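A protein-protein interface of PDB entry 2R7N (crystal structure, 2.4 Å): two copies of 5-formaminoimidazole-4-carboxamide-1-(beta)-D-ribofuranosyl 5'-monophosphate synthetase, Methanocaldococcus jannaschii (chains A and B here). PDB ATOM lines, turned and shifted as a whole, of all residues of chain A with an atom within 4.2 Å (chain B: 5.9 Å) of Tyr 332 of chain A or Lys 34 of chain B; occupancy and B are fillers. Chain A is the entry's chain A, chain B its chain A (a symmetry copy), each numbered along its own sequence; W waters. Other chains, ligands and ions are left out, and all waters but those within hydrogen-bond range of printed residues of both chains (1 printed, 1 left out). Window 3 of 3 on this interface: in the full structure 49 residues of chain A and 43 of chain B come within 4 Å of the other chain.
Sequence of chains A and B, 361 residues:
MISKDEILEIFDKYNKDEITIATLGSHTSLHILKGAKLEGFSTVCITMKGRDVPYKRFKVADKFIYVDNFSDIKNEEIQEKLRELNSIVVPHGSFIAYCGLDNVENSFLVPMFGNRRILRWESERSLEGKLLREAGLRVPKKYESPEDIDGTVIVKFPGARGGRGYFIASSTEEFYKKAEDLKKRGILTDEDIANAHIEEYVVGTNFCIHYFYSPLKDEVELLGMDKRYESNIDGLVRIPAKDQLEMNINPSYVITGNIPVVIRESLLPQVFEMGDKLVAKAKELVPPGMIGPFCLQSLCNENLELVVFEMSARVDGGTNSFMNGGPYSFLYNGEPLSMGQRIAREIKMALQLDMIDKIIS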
ATOM      1  N   GLU A 221      10.486  41.482   9.933  1.00  0.00           N
ATOM      2  CA  GLU A 221      10.623  40.154  10.526  1.00  0.00           C
ATOM      3  C   GLU A 221      11.498  40.230  11.768  1.00  0.00           C
ATOM      4  O   GLU A 221      12.435  41.026  11.829  1.00  0.00           O
ATOM      5  CB  GLU A 221      11.227  39.162   9.513  1.00  0.00           C
ATOM      6  CG  GLU A 221      10.420  39.012   8.223  1.00  0.00           C
ATOM      7  CD  GLU A 221      11.263  38.553   7.047  1.00  0.00           C
ATOM      8  OE1 GLU A 221      12.420  38.120   7.248  1.00  0.00           O
ATOM      9  OE2 GLU A 221      10.765  38.622   5.911  1.00  0.00           O
ATOM     10  N   LEU A 222      11.195  39.396  12.750  1.00  0.00           N
ATOM     11  CA  LEU A 222      12.059  39.246  13.903  1.00  0.00           C
ATOM     12  C   LEU A 222      12.994  38.071  13.694  1.00  0.00           C
ATOM     13  O   LEU A 222      12.550  36.930  13.567  1.00  0.00           O
ATOM     14  CB  LEU A 222      11.231  39.026  15.169  1.00  0.00           C
ATOM     15  CG  LEU A 222      11.998  38.810  16.480  1.00  0.00           C
ATOM     16  CD1 LEU A 222      12.999  39.918  16.728  1.00  0.00           C
ATOM     17  CD2 LEU A 222      10.996  38.731  17.598  1.00  0.00           C
ATOM     18  N   TYR A 328      14.082  32.417  17.197  1.00  0.00           N
ATOM     19  CA  TYR A 328      13.131  33.170  16.392  1.00  0.00           C
ATOM     20  C   TYR A 328      13.289  32.908  14.898  1.00  0.00           C
ATOM     21  O   TYR A 328      12.301  32.855  14.173  1.00  0.00           O
ATOM     22  CB  TYR A 328      13.237  34.673  16.690  1.00  0.00           C
ATOM     23  CG  TYR A 328      12.855  35.008  18.103  1.00  0.00           C
ATOM     24  CD1 TYR A 328      11.533  34.922  18.517  1.00  0.00           C
ATOM     25  CD2 TYR A 328      13.823  35.376  19.039  1.00  0.00           C
ATOM     26  CE1 TYR A 328      11.177  35.196  19.813  1.00  0.00           C
ATOM     27  CE2 TYR A 328      13.475  35.660  20.344  1.00  0.00           C
ATOM     28  CZ  TYR A 328      12.153  35.565  20.726  1.00  0.00           C
ATOM     29  OH  TYR A 328      11.792  35.839  22.014  1.00  0.00           O
ATOM     30  N   SER A 329      14.528  32.758  14.437  1.00  0.00           N
ATOM     31  CA  SER A 329      14.781  32.625  13.007  1.00  0.00           C
ATOM     32  C   SER A 329      14.289  31.252  12.549  1.00  0.00           C
ATOM     33  O   SER A 329      13.865  31.079  11.404  1.00  0.00           O
ATOM     34  CB  SER A 329      16.268  32.847  12.688  1.00  0.00           C
ATOM     35  OG  SER A 329      17.067  31.772  13.156  1.00  0.00           O
ATOM     36  N   PHE A 330      14.312  30.302  13.481  1.00  0.00           N
ATOM     37  CA  PHE A 330      13.819  28.943  13.286  1.00  0.00           C
ATOM     38  C   PHE A 330      12.335  28.873  12.930  1.00  0.00           C
ATOM     39  O   PHE A 330      11.920  28.071  12.101  1.00  0.00           O
ATOM     40  CB  PHE A 330      14.003  28.165  14.580  1.00  0.00           C
ATOM     41  CG  PHE A 330      13.635  26.709  14.471  1.00  0.00           C
ATOM     42  CD1 PHE A 330      14.517  25.798  13.913  1.00  0.00           C
ATOM     43  CD2 PHE A 330      12.419  26.253  14.941  1.00  0.00           C
ATOM     44  CE1 PHE A 330      14.182  24.457  13.812  1.00  0.00           C
ATOM     45  CE2 PHE A 330      12.077  24.912  14.844  1.00  0.00           C
ATOM     46  CZ  PHE A 330      12.954  24.017  14.286  1.00  0.00           C
ATOM     47  N   LEU A 331      11.541  29.691  13.603  1.00  0.00           N
ATOM     48  CA  LEU A 331      10.092  29.623  13.516  1.00  0.00           C
ATOM     49  C   LEU A 331       9.533  29.659  12.081  1.00  0.00           C
ATOM     50  O   LEU A 331       8.573  28.963  11.762  1.00  0.00           O
ATOM     51  CB  LEU A 331       9.495  30.745  14.366  1.00  0.00           C
ATOM     52  CG  LEU A 331       8.935  30.399  15.750  1.00  0.00           C
ATOM     53  CD1 LEU A 331       9.476  29.116  16.316  1.00  0.00           C
ATOM     54  CD2 LEU A 331       9.131  31.547  16.726  1.00  0.00           C
ATOM     55  N   TYR A 332      10.155  30.454  11.222  1.00  0.00           N
ATOM     56  CA  TYR A 332       9.716  30.627   9.849  1.00  0.00           C
ATOM     57  C   TYR A 332       9.650  29.326   9.051  1.00  0.00           C
ATOM     58  O   TYR A 332       8.609  28.981   8.481  1.00  0.00           O
ATOM     59  CB  TYR A 332      10.629  31.621   9.131  1.00  0.00           C
ATOM     60  CG  TYR A 332      10.586  33.002   9.732  1.00  0.00           C
ATOM     61  CD1 TYR A 332       9.509  33.846   9.491  1.00  0.00           C
ATOM     62  CD2 TYR A 332      11.623  33.468  10.549  1.00  0.00           C
ATOM     63  CE1 TYR A 332       9.460  35.116  10.040  1.00  0.00           C
ATOM     64  CE2 TYR A 332      11.585  34.747  11.106  1.00  0.00           C
ATOM     65  CZ  TYR A 332      10.498  35.562  10.844  1.00  0.00           C
ATOM     66  OH  TYR A 332      10.431  36.823  11.384  1.00  0.00           O
ATOM     67  N   ASN A 333      10.768  28.614   8.994  1.00  0.00           N
ATOM     68  CA  ASN A 333      10.839  27.395   8.186  1.00  0.00           C
ATOM     69  C   ASN A 333      11.542  26.233   8.881  1.00  0.00           C
ATOM     70  O   ASN A 333      11.937  25.278   8.231  1.00  0.00           O
ATOM     71  CB  ASN A 333      11.530  27.691   6.853  1.00  0.00           C
ATOM     72  CG  ASN A 333      10.763  28.696   6.006  1.00  0.00           C
ATOM     73  OD1 ASN A 333       9.587  28.503   5.705  1.00  0.00           O
ATOM     74  ND2 ASN A 333      11.431  29.776   5.620  1.00  0.00           N
ATOM     75  N   GLY A 334      11.715  26.325  10.198  1.00  0.00           N
ATOM     76  CA  GLY A 334      12.422  25.292  10.938  1.00  0.00           C
ATOM     77  C   GLY A 334      13.859  25.117  10.486  1.00  0.00           C
ATOM     78  O   GLY A 334      14.428  24.043  10.620  1.00  0.00           O
ATOM     79  N   SER B  29       3.446  30.006  23.146  1.00  0.00           N
ATOM     80  CA  SER B  29       2.674  29.458  22.033  1.00  0.00           C
ATOM     81  C   SER B  29       3.481  29.284  20.733  1.00  0.00           C
ATOM     82  O   SER B  29       3.329  28.288  20.033  1.00  0.00           O
ATOM     83  CB  SER B  29       1.417  30.286  21.787  1.00  0.00           C
ATOM     84  OG  SER B  29       1.759  31.572  21.292  1.00  0.00           O
ATOM     85  N   LEU B  30       4.334  30.250  20.418  1.00  0.00           N
ATOM     86  CA  LEU B  30       5.133  30.202  19.194  1.00  0.00           C
ATOM     87  C   LEU B  30       5.695  28.818  18.902  1.00  0.00           C
ATOM     88  O   LEU B  30       5.547  28.328  17.792  1.00  0.00           O
ATOM     89  CB  LEU B  30       6.257  31.234  19.228  1.00  0.00           C
ATOM     90  CG  LEU B  30       5.687  32.641  19.106  1.00  0.00           C
ATOM     91  CD1 LEU B  30       6.762  33.673  19.215  1.00  0.00           C
ATOM     92  CD2 LEU B  30       4.948  32.790  17.800  1.00  0.00           C
ATOM     93  N   HIS B  31       6.317  28.185  19.890  1.00  0.00           N
ATOM     94  CA  HIS B  31       6.864  26.847  19.687  1.00  0.00           C
ATOM     95  C   HIS B  31       5.882  25.709  20.000  1.00  0.00           C
ATOM     96  O   HIS B  31       6.108  24.564  19.614  1.00  0.00           O
ATOM     97  CB  HIS B  31       8.188  26.654  20.454  1.00  0.00           C
ATOM     98  CG  HIS B  31       8.040  26.656  21.943  1.00  0.00           C
ATOM     99  ND1 HIS B  31       7.742  25.518  22.662  1.00  0.00           N
ATOM    100  CD2 HIS B  31       8.168  27.654  22.851  1.00  0.00           C
ATOM    101  CE1 HIS B  31       7.676  25.816  23.949  1.00  0.00           C
ATOM    102  NE2 HIS B  31       7.936  27.105  24.090  1.00  0.00           N
ATOM    103  N   ILE B  32       4.816  26.013  20.727  1.00  0.00           N
ATOM    104  CA  ILE B  32       3.719  25.083  20.873  1.00  0.00           C
ATOM    105  C   ILE B  32       3.056  24.938  19.509  1.00  0.00           C
ATOM    106  O   ILE B  32       2.746  23.829  19.063  1.00  0.00           O
ATOM    107  CB  ILE B  32       2.659  25.617  21.871  1.00  0.00           C
ATOM    108  CG1 ILE B  32       3.085  25.341  23.315  1.00  0.00           C
ATOM    109  CG2 ILE B  32       1.286  25.004  21.593  1.00  0.00           C
ATOM    110  CD1 ILE B  32       2.332  26.192  24.340  1.00  0.00           C
ATOM    111  N   LEU B  33       2.830  26.072  18.852  1.00  0.00           N
ATOM    112  CA  LEU B  33       2.181  26.072  17.556  1.00  0.00           C
ATOM    113  C   LEU B  33       3.136  25.545  16.474  1.00  0.00           C
ATOM    114  O   LEU B  33       2.796  24.631  15.726  1.00  0.00           O
ATOM    115  CB  LEU B  33       1.670  27.469  17.210  1.00  0.00           C
ATOM    116  CG  LEU B  33       0.564  28.071  18.086  1.00  0.00           C
ATOM    117  CD1 LEU B  33       0.210  29.477  17.610  1.00  0.00           C
ATOM    118  CD2 LEU B  33      -0.675  27.185  18.144  1.00  0.00           C
ATOM    119  N   LYS B  34       4.338  26.106  16.409  1.00  0.00           N
ATOM    120  CA  LYS B  34       5.341  25.635  15.457  1.00  0.00           C
ATOM    121  C   LYS B  34       5.616  24.150  15.619  1.00  0.00           C
ATOM    122  O   LYS B  34       5.841  23.444  14.640  1.00  0.00           O
ATOM    123  CB  LYS B  34       6.643  26.403  15.615  1.00  0.00           C
ATOM    124  CG  LYS B  34       7.723  25.999  14.657  1.00  0.00           C
ATOM    125  CD  LYS B  34       7.305  26.251  13.236  1.00  0.00           C
ATOM    126  CE  LYS B  34       8.443  25.933  12.288  1.00  0.00           C
ATOM    127  NZ  LYS B  34       8.261  26.667  11.015  1.00  0.00           N
ATOM    128  N   GLY B  35       5.595  23.679  16.855  1.00  0.00           N
ATOM    129  CA  GLY B  35       5.897  22.277  17.121  1.00  0.00           C
ATOM    130  C   GLY B  35       4.795  21.357  16.643  1.00  0.00           C
ATOM    131  O   GLY B  35       5.043  20.221  16.262  1.00  0.00           O
ATOM    132  N   ALA B  36       3.567  21.856  16.688  1.00  0.00           N
ATOM    133  CA  ALA B  36       2.416  21.150  16.152  1.00  0.00           C
ATOM    134  C   ALA B  36       2.537  21.033  14.628  1.00  0.00           C
ATOM    135  O   ALA B  36       2.441  19.953  14.069  1.00  0.00           O
ATOM    136  CB  ALA B  36       1.152  21.892  16.524  1.00  0.00           C
ATOM    137  N   LYS B  37       2.738  22.161  13.970  1.00  0.00           N
ATOM    138  CA  LYS B  37       2.948  22.190  12.545  1.00  0.00           C
ATOM    139  C   LYS B  37       4.002  21.179  12.117  1.00  0.00           C
ATOM    140  O   LYS B  37       3.808  20.461  11.142  1.00  0.00           O
ATOM    141  CB  LYS B  37       3.384  23.592  12.117  1.00  0.00           C
ATOM    142  CG  LYS B  37       2.363  24.667  12.418  1.00  0.00           C
ATOM    143  CD  LYS B  37       1.239  24.653  11.412  1.00  0.00           C
ATOM    144  CE  LYS B  37       1.759  24.983  10.032  1.00  0.00           C
ATOM    145  NZ  LYS B  37       0.640  25.189   9.073  1.00  0.00           N
ATOM    146  N   LEU B  38       5.114  21.130  12.846  1.00  0.00           N
ATOM    147  CA  LEU B  38       6.229  20.259  12.499  1.00  0.00           C
ATOM    148  C   LEU B  38       5.850  18.796  12.673  1.00  0.00           C
ATOM    149  O   LEU B  38       6.483  17.916  12.095  1.00  0.00           O
ATOM    150  CB  LEU B  38       7.468  20.580  13.344  1.00  0.00           C
ATOM    151  CG  LEU B  38       8.216  21.881  13.037  1.00  0.00           C
ATOM    152  CD1 LEU B  38       9.162  22.209  14.157  1.00  0.00           C
ATOM    153  CD2 LEU B  38       8.969  21.810  11.711  1.00  0.00           C
ATOM    154  N   GLU B  39       4.826  18.532  13.477  1.00  0.00           N
ATOM    155  CA  GLU B  39       4.379  17.154  13.687  1.00  0.00           C
ATOM    156  C   GLU B  39       3.198  16.807  12.786  1.00  0.00           C
ATOM    157  O   GLU B  39       2.661  15.699  12.853  1.00  0.00           O
ATOM    158  CB  GLU B  39       4.029  16.907  15.152  1.00  0.00           C
ATOM    159  CG  GLU B  39       5.242  16.888  16.075  1.00  0.00           C
ATOM    160  CD  GLU B  39       6.177  15.730  15.799  1.00  0.00           C
ATOM    161  OE1 GLU B  39       5.719  14.568  15.841  1.00  0.00           O
ATOM    162  OE2 GLU B  39       7.378  15.975  15.550  1.00  0.00           O
ATOM    163  N   THR B  43      -2.857  24.105  13.329  1.00  0.00           N
ATOM    164  CA  THR B  43      -2.808  24.805  14.601  1.00  0.00           C
ATOM    165  C   THR B  43      -3.810  25.931  14.709  1.00  0.00           C
ATOM    166  O   THR B  43      -4.010  26.701  13.763  1.00  0.00           O
ATOM    167  CB  THR B  43      -1.433  25.434  14.832  1.00  0.00           C
ATOM    168  OG1 THR B  43      -1.133  26.311  13.743  1.00  0.00           O
ATOM    169  CG2 THR B  43      -0.376  24.378  14.948  1.00  0.00           C
ATOM    170  N   ARG B  57       3.303  36.859  11.525  1.00  0.00           N
ATOM    171  CA  ARG B  57       4.589  36.965  10.839  1.00  0.00           C
ATOM    172  C   ARG B  57       5.420  35.698  11.032  1.00  0.00           C
ATOM    173  O   ARG B  57       6.341  35.427  10.270  1.00  0.00           O
ATOM    174  CB  ARG B  57       5.376  38.187  11.324  1.00  0.00           C
ATOM    175  CG  ARG B  57       4.552  39.446  11.475  1.00  0.00           C
ATOM    176  CD  ARG B  57       4.828  40.458  10.386  1.00  0.00           C
ATOM    177  NE  ARG B  57       4.191  41.734  10.701  1.00  0.00           N
ATOM    178  CZ  ARG B  57       4.834  42.886  10.872  1.00  0.00           C
ATOM    179  NH1 ARG B  57       6.150  42.950  10.734  1.00  0.00           N
ATOM    180  NH2 ARG B  57       4.153  43.980  11.167  1.00  0.00           N
ATOM    181  N   PHE B  58       5.126  34.925  12.064  1.00  0.00           N
ATOM    182  CA  PHE B  58       5.868  33.678  12.224  1.00  0.00           C
ATOM    183  C   PHE B  58       5.184  32.488  11.529  1.00  0.00           C
ATOM    184  O   PHE B  58       5.736  31.395  11.498  1.00  0.00           O
ATOM    185  CB  PHE B  58       6.182  33.387  13.697  1.00  0.00           C
ATOM    186  CG  PHE B  58       7.347  34.180  14.240  1.00  0.00           C
ATOM    187  CD1 PHE B  58       8.586  34.130  13.618  1.00  0.00           C
ATOM    188  CD2 PHE B  58       7.206  34.963  15.380  1.00  0.00           C
ATOM    189  CE1 PHE B  58       9.656  34.846  14.116  1.00  0.00           C
ATOM    190  CE2 PHE B  58       8.279  35.682  15.889  1.00  0.00           C
ATOM    191  CZ  PHE B  58       9.502  35.624  15.258  1.00  0.00           C
ATOM    192  N   LYS B  59       3.994  32.724  10.971  1.00  0.00           N
ATOM    193  CA  LYS B  59       3.293  31.765  10.102  1.00  0.00           C
ATOM    194  C   LYS B  59       3.097  30.443  10.819  1.00  0.00           C
ATOM    195  O   LYS B  59       3.344  29.375  10.276  1.00  0.00           O
ATOM    196  CB  LYS B  59       4.064  31.546   8.796  1.00  0.00           C
ATOM    197  CG  LYS B  59       4.249  32.802   7.942  1.00  0.00           C
ATOM    198  CD  LYS B  59       2.907  33.381   7.517  1.00  0.00           C
ATOM    199  CE  LYS B  59       3.079  34.743   6.845  1.00  0.00           C
ATOM    200  NZ  LYS B  59       1.791  35.491   6.807  1.00  0.00           N
ATOM    201  N   VAL B  60       2.629  30.535  12.050  1.00  0.00           N
ATOM    202  CA  VAL B  60       2.759  29.459  12.995  1.00  0.00           C
ATOM    203  C   VAL B  60       1.369  28.958  13.312  1.00  0.00           C
ATOM    204  O   VAL B  60       1.194  27.877  13.865  1.00  0.00           O
ATOM    205  CB  VAL B  60       3.492  29.995  14.268  1.00  0.00           C
ATOM    206  CG1 VAL B  60       2.538  30.157  15.446  1.00  0.00           C
ATOM    207  CG2 VAL B  60       4.679  29.130  14.618  1.00  0.00           C
ATOM    208  N   SER B 338      11.964  21.371  20.086  1.00  0.00           N
ATOM    209  CA  SER B 338      11.429  22.282  21.088  1.00  0.00           C
ATOM    210  C   SER B 338      10.484  21.528  22.004  1.00  0.00           C
ATOM    211  O   SER B 338      10.150  20.381  21.746  1.00  0.00           O
ATOM    212  CB  SER B 338      10.661  23.412  20.421  1.00  0.00           C
ATOM    213  OG  SER B 338       9.423  22.930  19.930  1.00  0.00           O
ATOM    214  N   GLN B 341       7.052  21.038  20.313  1.00  0.00           N
ATOM    215  CA  GLN B 341       7.046  19.911  19.403  1.00  0.00           C
ATOM    216  C   GLN B 341       7.014  18.594  20.159  1.00  0.00           C
ATOM    217  O   GLN B 341       6.305  17.672  19.776  1.00  0.00           O
ATOM    218  CB  GLN B 341       8.259  19.931  18.467  1.00  0.00           C
ATOM    219  CG  GLN B 341       8.263  18.735  17.525  1.00  0.00           C
ATOM    220  CD  GLN B 341       9.336  18.796  16.445  1.00  0.00           C
ATOM    221  OE1 GLN B 341      10.260  19.618  16.494  1.00  0.00           O
ATOM    222  NE2 GLN B 341       9.213  17.911  15.454  1.00  0.00           N
HETATM  223  O   HOH W   1       9.008  24.328   8.733  1.00  0.00           O
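The backbone carbonyl oxygen of Leu 331 of chain A sits at hydrogen-bond distance from the side-chain amino group of Lys 34 of chain B (2.4 Å). The side-chain amino group (NZ) of Lys 34 of chain B is in hydrogen-bond range of the backbone carbonyl oxygen (O) of Tyr 332 of chain A (3.4 Å).
The side-chain hydroxyl of Tyr 332 of chain A lies within hydrogen-bond range of the backbone NH of Leu 222 of chain A (3.0 Å).
Among the printed residues, merely in contact across the chains: Tyr 332 of chain A with Arg 57 of chain B (3.1 Å), Tyr 328 of chain A with Phe 58 of chain B (3.3 Å), Tyr 332 of chain A with Phe 58 of chain B (3.5 Å), Gly 334 of chain A with Lys 34 of chain B (3.6 Å), Leu 331 of chain A with Phe 58 of chain B (3.6 Å), Leu 222 of chain A with Phe 58 of chain B (3.6 Å), Asn 333 of chain A with Lys 34 of chain B (3.8 Å) and Leu 331 of chain A with Leu 30 of chain B (3.8 Å).
Of chain A, only Leu 331 (2.4 Å), Tyr 332 (3.4 Å), Asn 333 (3.8 Å) and Gly 334 (3.6 Å) come within 4 Å of Lys 34 of chain B. Of the printed residues of chain A, Phe 58 of chain B touches Leu 222, Tyr 328, Leu 331 and Tyr 332. Of the printed residues of chain A, Leu 30 of chain B touches Leu 331. The nearest residue of chain A that does not touch Lys 34 of chain B is Phe 330 of chain A (4.1 Å). The nearest printed residue of chain B that does not touch Gly 334 of chain A is Leu 38 of chain B (5.0 Å).
Hydrophobic or aromatic side chains of chain A within 4 Å of the printed part of chain B: Leu 222, Tyr 328, Leu 331 and Tyr 332. Of the 18 printed residues of chain B, 4 touch a printed residue of chain A. Hydrophobic or aromatic side chains of chain B within 4 Å of the printed part of chain A: Leu 30 and Phe 58.
No position is printed for both chains. Of the 10 pairs that touch across the chains among the printed residues, none has its exchanged pair printed and touching as well.
Water W1 bridges O of Asn 333 of chain A (3.1 Å) and NZ of Lys 34 of chain B (3.4 Å).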
